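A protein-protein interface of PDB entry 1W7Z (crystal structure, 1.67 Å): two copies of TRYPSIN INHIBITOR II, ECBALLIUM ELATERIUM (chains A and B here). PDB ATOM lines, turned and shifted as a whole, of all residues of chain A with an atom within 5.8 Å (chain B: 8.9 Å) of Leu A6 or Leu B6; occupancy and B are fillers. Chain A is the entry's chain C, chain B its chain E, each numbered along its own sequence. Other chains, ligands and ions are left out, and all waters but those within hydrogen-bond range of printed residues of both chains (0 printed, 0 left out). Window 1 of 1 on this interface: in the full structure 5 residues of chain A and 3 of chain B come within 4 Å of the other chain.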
ATOM      1  N   ARG A   4      24.074 -38.104  26.711  1.00  0.00           N
ATOM      2  CA  ARG A   4      23.055 -37.484  25.895  1.00  0.00           C
ATOM      3  C   ARG A   4      22.580 -36.072  26.369  1.00  0.00           C
ATOM      4  O   ARG A   4      21.580 -35.505  25.822  1.00  0.00           O
ATOM      5  CB  ARG A   4      21.888 -38.494  25.656  1.00  0.00           C
ATOM      6  CG  ARG A   4      22.231 -39.478  24.470  1.00  0.00           C
ATOM      7  CD  ARG A   4      21.050 -39.902  23.550  1.00  0.00           C
ATOM      8  NE  ARG A   4      20.633 -39.071  22.360  1.00  0.00           N
ATOM      9  CZ  ARG A   4      21.312 -38.131  21.715  1.00  0.00           C
ATOM     10  NH1 ARG A   4      22.553 -37.724  22.046  1.00  0.00           N
ATOM     11  NH2 ARG A   4      20.721 -37.540  20.691  1.00  0.00           N
ATOM     12  N   ILE A   5      23.376 -35.448  27.251  1.00  0.00           N
ATOM     13  CA  ILE A   5      23.165 -34.058  27.629  1.00  0.00           C
ATOM     14  C   ILE A   5      23.448 -33.197  26.409  1.00  0.00           C
ATOM     15  O   ILE A   5      24.465 -33.416  25.715  1.00  0.00           O
ATOM     16  CB  ILE A   5      24.129 -33.652  28.788  1.00  0.00           C
ATOM     17  CG1 ILE A   5      23.940 -34.629  29.978  1.00  0.00           C
ATOM     18  CG2 ILE A   5      23.991 -32.197  29.159  1.00  0.00           C
ATOM     19  CD1 ILE A   5      25.097 -34.666  30.931  1.00  0.00           C
ATOM     20  N   LEU A   6      22.600 -32.217  26.131  1.00  0.00           N
ATOM     21  CA  LEU A   6      22.857 -31.328  24.971  1.00  0.00           C
ATOM     22  C   LEU A   6      23.932 -30.307  25.358  1.00  0.00           C
ATOM     23  O   LEU A   6      23.755 -29.536  26.323  1.00  0.00           O
ATOM     24  CB  LEU A   6      21.599 -30.578  24.576  1.00  0.00           C
ATOM     25  CG  LEU A   6      20.704 -31.262  23.568  1.00  0.00           C
ATOM     26  CD1 LEU A   6      20.151 -32.461  24.188  1.00  0.00           C
ATOM     27  CD2 LEU A   6      19.644 -30.356  23.085  1.00  0.00           C
ATOM     28  N   ILE A   7      25.054 -30.337  24.641  1.00  0.00           N
ATOM     29  CA  ILE A   7      26.168 -29.416  24.877  1.00  0.00           C
ATOM     30  C   ILE A   7      26.557 -28.844  23.512  1.00  0.00           C
ATOM     31  O   ILE A   7      26.863 -29.596  22.603  1.00  0.00           O
ATOM     32  CB  ILE A   7      27.338 -30.136  25.523  1.00  0.00           C
ATOM     33  CG1 ILE A   7      26.864 -30.822  26.760  1.00  0.00           C
ATOM     34  CG2 ILE A   7      28.509 -29.199  25.809  1.00  0.00           C
ATOM     35  CD1 ILE A   7      27.957 -31.476  27.605  1.00  0.00           C
ATOM     36  N   ARG A   8      26.499 -27.546  23.368  1.00  0.00           N
ATOM     37  CA  ARG A   8      27.005 -26.899  22.147  1.00  0.00           C
ATOM     38  C   ARG A   8      28.550 -26.937  22.115  1.00  0.00           C
ATOM     39  O   ARG A   8      29.204 -26.792  23.122  1.00  0.00           O
ATOM     40  CB  ARG A   8      26.489 -25.445  22.040  1.00  0.00           C
ATOM     41  CG  ARG A   8      25.038 -25.378  21.761  1.00  0.00           C
ATOM     42  CD  ARG A   8      24.548 -24.036  21.225  1.00  0.00           C
ATOM     43  NE  ARG A   8      23.410 -24.246  20.332  1.00  0.00           N
ATOM     44  CZ  ARG A   8      22.154 -23.867  20.542  1.00  0.00           C
ATOM     45  NH1 ARG A   8      21.778 -23.225  21.655  1.00  0.00           N
ATOM     46  NH2 ARG A   8      21.243 -24.146  19.602  1.00  0.00           N
ATOM     47  N   PHE A  26      26.425 -29.783  18.088  1.00  0.00           N
ATOM     48  CA  PHE A  26      26.233 -30.407  19.408  1.00  0.00           C
ATOM     49  C   PHE A  26      27.152 -31.582  19.567  1.00  0.00           C
ATOM     50  O   PHE A  26      27.455 -32.284  18.598  1.00  0.00           O
ATOM     51  CB  PHE A  26      24.785 -30.927  19.508  1.00  0.00           C
ATOM     52  CG  PHE A  26      23.794 -29.830  19.730  1.00  0.00           C
ATOM     53  CD1 PHE A  26      23.029 -29.341  18.673  1.00  0.00           C
ATOM     54  CD2 PHE A  26      23.628 -29.288  20.975  1.00  0.00           C
ATOM     55  CE1 PHE A  26      22.145 -28.318  18.862  1.00  0.00           C
ATOM     56  CE2 PHE A  26      22.772 -28.244  21.177  1.00  0.00           C
ATOM     57  CZ  PHE A  26      22.000 -27.761  20.125  1.00  0.00           C
ATOM     58  N   CYS B   2      30.264 -19.162  30.764  1.00  0.00           N
ATOM     59  CA  CYS B   2      29.166 -19.995  31.153  1.00  0.00           C
ATOM     60  C   CYS B   2      29.381 -21.385  30.495  1.00  0.00           C
ATOM     61  O   CYS B   2      29.896 -21.429  29.424  1.00  0.00           O
ATOM     62  CB  CYS B   2      27.966 -19.221  30.654  1.00  0.00           C
ATOM     63  SG  CYS B   2      26.449 -19.857  30.825  1.00  0.00           S
ATOM     64  N   PRO B   3      29.012 -22.509  31.142  1.00  0.00           N
ATOM     65  CA  PRO B   3      29.112 -23.800  30.426  1.00  0.00           C
ATOM     66  C   PRO B   3      28.157 -23.790  29.224  1.00  0.00           C
ATOM     67  O   PRO B   3      27.168 -23.072  29.255  1.00  0.00           O
ATOM     68  CB  PRO B   3      28.636 -24.817  31.440  1.00  0.00           C
ATOM     69  CG  PRO B   3      28.665 -24.103  32.730  1.00  0.00           C
ATOM     70  CD  PRO B   3      28.489 -22.681  32.499  1.00  0.00           C
ATOM     71  N   ARG B   4      28.443 -24.582  28.188  1.00  0.00           N
ATOM     72  CA  ARG B   4      27.675 -24.599  26.988  1.00  0.00           C
ATOM     73  C   ARG B   4      26.658 -25.765  26.996  1.00  0.00           C
ATOM     74  O   ARG B   4      26.100 -26.122  25.983  1.00  0.00           O
ATOM     75  CB  ARG B   4      28.603 -24.803  25.795  1.00  0.00           C
ATOM     76  CG  ARG B   4      29.549 -23.652  25.533  1.00  0.00           C
ATOM     77  CD  ARG B   4      28.892 -22.606  24.668  1.00  0.00           C
ATOM     78  NE  ARG B   4      28.830 -22.965  23.246  1.00  0.00           N
ATOM     79  CZ  ARG B   4      28.120 -22.285  22.347  1.00  0.00           C
ATOM     80  NH1 ARG B   4      28.111 -22.658  21.074  1.00  0.00           N
ATOM     81  NH2 ARG B   4      27.376 -21.253  22.717  1.00  0.00           N
ATOM     82  N   ILE B   5      26.430 -26.311  28.178  1.00  0.00           N
ATOM     83  CA  ILE B   5      25.312 -27.213  28.409  1.00  0.00           C
ATOM     84  C   ILE B   5      24.009 -26.462  28.254  1.00  0.00           C
ATOM     85  O   ILE B   5      23.843 -25.366  28.770  1.00  0.00           O
ATOM     86  CB  ILE B   5      25.368 -27.777  29.864  1.00  0.00           C
ATOM     87  CG1 ILE B   5      26.656 -28.535  30.112  1.00  0.00           C
ATOM     88  CG2 ILE B   5      24.134 -28.602  30.133  1.00  0.00           C
ATOM     89  CD1 ILE B   5      26.970 -28.724  31.539  1.00  0.00           C
ATOM     90  N   LEU B   6      23.060 -27.053  27.551  1.00  0.00           N
ATOM     91  CA  LEU B   6      21.744 -26.413  27.353  1.00  0.00           C
ATOM     92  C   LEU B   6      20.884 -26.569  28.603  1.00  0.00           C
ATOM     93  O   LEU B   6      20.572 -27.649  29.028  1.00  0.00           O
ATOM     94  CB  LEU B   6      21.044 -26.915  26.087  1.00  0.00           C
ATOM     95  CG  LEU B   6      21.558 -26.360  24.749  1.00  0.00           C
ATOM     96  CD1 LEU B   6      20.490 -26.669  23.641  1.00  0.00           C
ATOM     97  CD2 LEU B   6      21.878 -24.893  24.822  1.00  0.00           C
ATOM     98  N   ILE B   7      20.582 -25.461  29.244  1.00  0.00           N
ATOM     99  CA  ILE B   7      19.720 -25.410  30.414  1.00  0.00           C
ATOM    100  C   ILE B   7      18.626 -24.388  30.162  1.00  0.00           C
ATOM    101  O   ILE B   7      18.899 -23.228  29.906  1.00  0.00           O
ATOM    102  CB  ILE B   7      20.546 -25.031  31.672  1.00  0.00           C
ATOM    103  CG1 ILE B   7      21.730 -26.001  31.797  1.00  0.00           C
ATOM    104  CG2 ILE B   7      19.697 -25.066  32.911  1.00  0.00           C
ATOM    105  CD1 ILE B   7      22.542 -25.742  33.042  1.00  0.00           C
ATOM    106  N   ARG B   8      17.379 -24.804  30.275  1.00  0.00           N
ATOM    107  CA  ARG B   8      16.268 -23.884  30.059  1.00  0.00           C
ATOM    108  C   ARG B   8      16.115 -23.049  31.297  1.00  0.00           C
ATOM    109  O   ARG B   8      16.405 -23.522  32.408  1.00  0.00           O
ATOM    110  CB  ARG B   8      14.985 -24.671  29.783  1.00  0.00           C
ATOM    111  CG  ARG B   8      14.929 -25.016  28.392  1.00  0.00           C
ATOM    112  CD  ARG B   8      13.503 -25.279  28.022  1.00  0.00           C
ATOM    113  NE  ARG B   8      13.134 -26.619  28.387  1.00  0.00           N
ATOM    114  CZ  ARG B   8      11.890 -27.084  28.304  1.00  0.00           C
ATOM    115  NH1 ARG B   8      10.897 -26.260  27.938  1.00  0.00           N
ATOM    116  NH2 ARG B   8      11.655 -28.361  28.632  1.00  0.00           N
ATOM    117  N   CYS B   9      15.707 -21.796  31.106  1.00  0.00           N
ATOM    118  CA  CYS B   9      15.627 -20.879  32.194  1.00  0.00           C
ATOM    119  C   CYS B   9      14.503 -19.878  31.986  1.00  0.00           C
ATOM    120  O   CYS B   9      14.133 -19.539  30.841  1.00  0.00           O
ATOM    121  CB  CYS B   9      16.954 -20.148  32.372  1.00  0.00           C
ATOM    122  SG  CYS B   9      17.510 -19.238  30.898  1.00  0.00           S
ATOM    123  N   CYS B  15      20.335 -20.291  36.280  1.00  0.00           N
ATOM    124  CA  CYS B  15      21.573 -20.636  35.624  1.00  0.00           C
ATOM    125  C   CYS B  15      22.788 -20.810  36.521  1.00  0.00           C
ATOM    126  O   CYS B  15      22.811 -20.340  37.665  1.00  0.00           O
ATOM    127  CB  CYS B  15      21.841 -19.540  34.578  1.00  0.00           C
ATOM    128  SG  CYS B  15      20.460 -19.355  33.353  1.00  0.00           S
ATOM    129  N   LEU B  16      23.810 -21.459  35.980  1.00  0.00           N
ATOM    130  CA  LEU B  16      25.093 -21.631  36.675  1.00  0.00           C
ATOM    131  C   LEU B  16      25.848 -20.320  36.769  1.00  0.00           C
ATOM    132  O   LEU B  16      25.455 -19.314  36.144  1.00  0.00           O
ATOM    133  CB  LEU B  16      25.901 -22.738  35.939  1.00  0.00           C
ATOM    134  CG  LEU B  16      25.157 -24.083  35.992  1.00  0.00           C
ATOM    135  CD1 LEU B  16      25.886 -25.109  35.180  1.00  0.00           C
ATOM    136  CD2 LEU B  16      24.986 -24.617  37.403  1.00  0.00           C
ATOM    137  N   ASN B  24      17.037 -16.364  23.990  1.00  0.00           N
ATOM    138  CA  ASN B  24      16.695 -17.710  23.495  1.00  0.00           C
ATOM    139  C   ASN B  24      16.053 -18.658  24.536  1.00  0.00           C
ATOM    140  O   ASN B  24      15.645 -19.747  24.177  1.00  0.00           O
ATOM    141  CB  ASN B  24      17.913 -18.407  22.829  1.00  0.00           C
ATOM    142  CG  ASN B  24      19.078 -18.612  23.767  1.00  0.00           C
ATOM    143  OD1 ASN B  24      19.096 -18.104  24.902  1.00  0.00           O
ATOM    144  ND2 ASN B  24      20.088 -19.351  23.291  1.00  0.00           N
ATOM    145  N   GLY B  25      15.933 -18.252  25.804  1.00  0.00           N
ATOM    146  CA  GLY B  25      15.252 -19.074  26.806  1.00  0.00           C
ATOM    147  C   GLY B  25      16.221 -20.107  27.425  1.00  0.00           C
ATOM    148  O   GLY B  25      15.790 -21.002  28.140  1.00  0.00           O
ATOM    149  N   PHE B  26      17.514 -19.943  27.158  1.00  0.00           N
ATOM    150  CA  PHE B  26      18.567 -20.823  27.684  1.00  0.00           C
ATOM    151  C   PHE B  26      19.592 -19.978  28.406  1.00  0.00           C
ATOM    152  O   PHE B  26      19.806 -18.809  28.053  1.00  0.00           O
ATOM    153  CB  PHE B  26      19.310 -21.585  26.556  1.00  0.00           C
ATOM    154  CG  PHE B  26      18.468 -22.607  25.860  1.00  0.00           C
ATOM    155  CD1 PHE B  26      17.979 -22.383  24.596  1.00  0.00           C
ATOM    156  CD2 PHE B  26      18.184 -23.802  26.454  1.00  0.00           C
ATOM    157  CE1 PHE B  26      17.215 -23.339  23.954  1.00  0.00           C
ATOM    158  CE2 PHE B  26      17.412 -24.723  25.841  1.00  0.00           C
ATOM    159  CZ  PHE B  26      16.892 -24.477  24.585  1.00  0.00           C
ATOM    160  N   CYS B  27      20.285 -20.567  29.355  1.00  0.00           N
ATOM    161  CA  CYS B  27      21.423 -19.959  30.041  1.00  0.00           C
ATOM    162  C   CYS B  27      22.570 -19.733  29.099  1.00  0.00           C
ATOM    163  O   CYS B  27      22.908 -20.615  28.262  1.00  0.00           O
ATOM    164  CB  CYS B  27      21.889 -20.901  31.149  1.00  0.00           C
ATOM    165  SG  CYS B  27      20.541 -21.176  32.353  1.00  0.00           S
ATOM    166  N   GLY B  28      23.196 -18.564  29.224  1.00  0.00           N
ATOM    167  CA  GLY B  28      24.349 -18.243  28.393  1.00  0.00           C
ATOM    168  C   GLY B  28      25.230 -17.191  29.012  1.00  0.00           C
ATOM    169  O   GLY B  28      24.925 -16.656  30.095  1.00  0.00           O
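The backbone NH of Leu B6 lies within hydrogen-bond range of the backbone carbonyl oxygen of Leu A6. The backbone NH (N) of Arg A8 is in hydrogen-bond range of the backbone carbonyl oxygen (O) of Arg B4 (3.0 Å).
The side-chain sulfur (SG) of Cys B15 forms a disulfide with the side-chain sulfur (SG) of Cys B27 (2.1 Å).
Among the printed residues, pairs that only touch across the chains: Ile A5 with Ile B5, Leu A6 with Ile B5, Ile A7 with Arg B4, Arg A8 with Leu B6 and Phe A26 with Leu B6.
Of the printed residues of chain B, Ile A5 touches Ile B5. Printed residues of chain B within 4 Å of Leu A6: Ile B5 (3.5 Å) and Leu B6 (2.9 Å). Of the printed residues of chain B, Ile A7 touches Arg B4. Printed residues of chain B within 4 Å of Arg A8: Arg B4 and Leu B6. Of the printed residues of chain A, Arg B4 touches Ile A7 and Arg A8. Of the printed residues of chain A, Leu B6 touches Leu A6 (2.9 Å), Arg A8 (3.6 Å) and Phe A26 (3.7 Å). The nearest printed residue of chain B that does not touch Ile A7 is Ile B5 (4.1 Å).
Of the 15 printed residues of chain B, 3 touch a printed residue of chain A. Hydrophobic or aromatic side chains of chain B that line the printed part of chain A: Ile B5 and Leu B6. Of the 6 printed residues of chain A, 5 touch a printed residue of chain B. Hydrophobic or aromatic side chains of chain A within 4 Å of the printed part of chain B: Ile A5, Leu A6, Ile A7 and Phe A26. Among the printed residues, 7 pairs touch across the chains.
Leu A6 touches Ile B5, but with the chains exchanged Ile A5 does not touch Leu B6 (5.5 Å). Leu B6 touches its own counterpart, Leu A6. Arg A8 touches Arg B4, but with the chains exchanged Arg A4 does not touch Arg B8 (12.3 Å). Arg A8 touches Leu B6, but with the chains exchanged Leu A6 does not touch Arg B8 (8.9 Å). Positions printed for both chains: 4, 5, 6, 7, 8 and 26. Of the 7 pairs that touch across the chains among the printed residues, 2 have their exchanged pair printed and touching as well.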
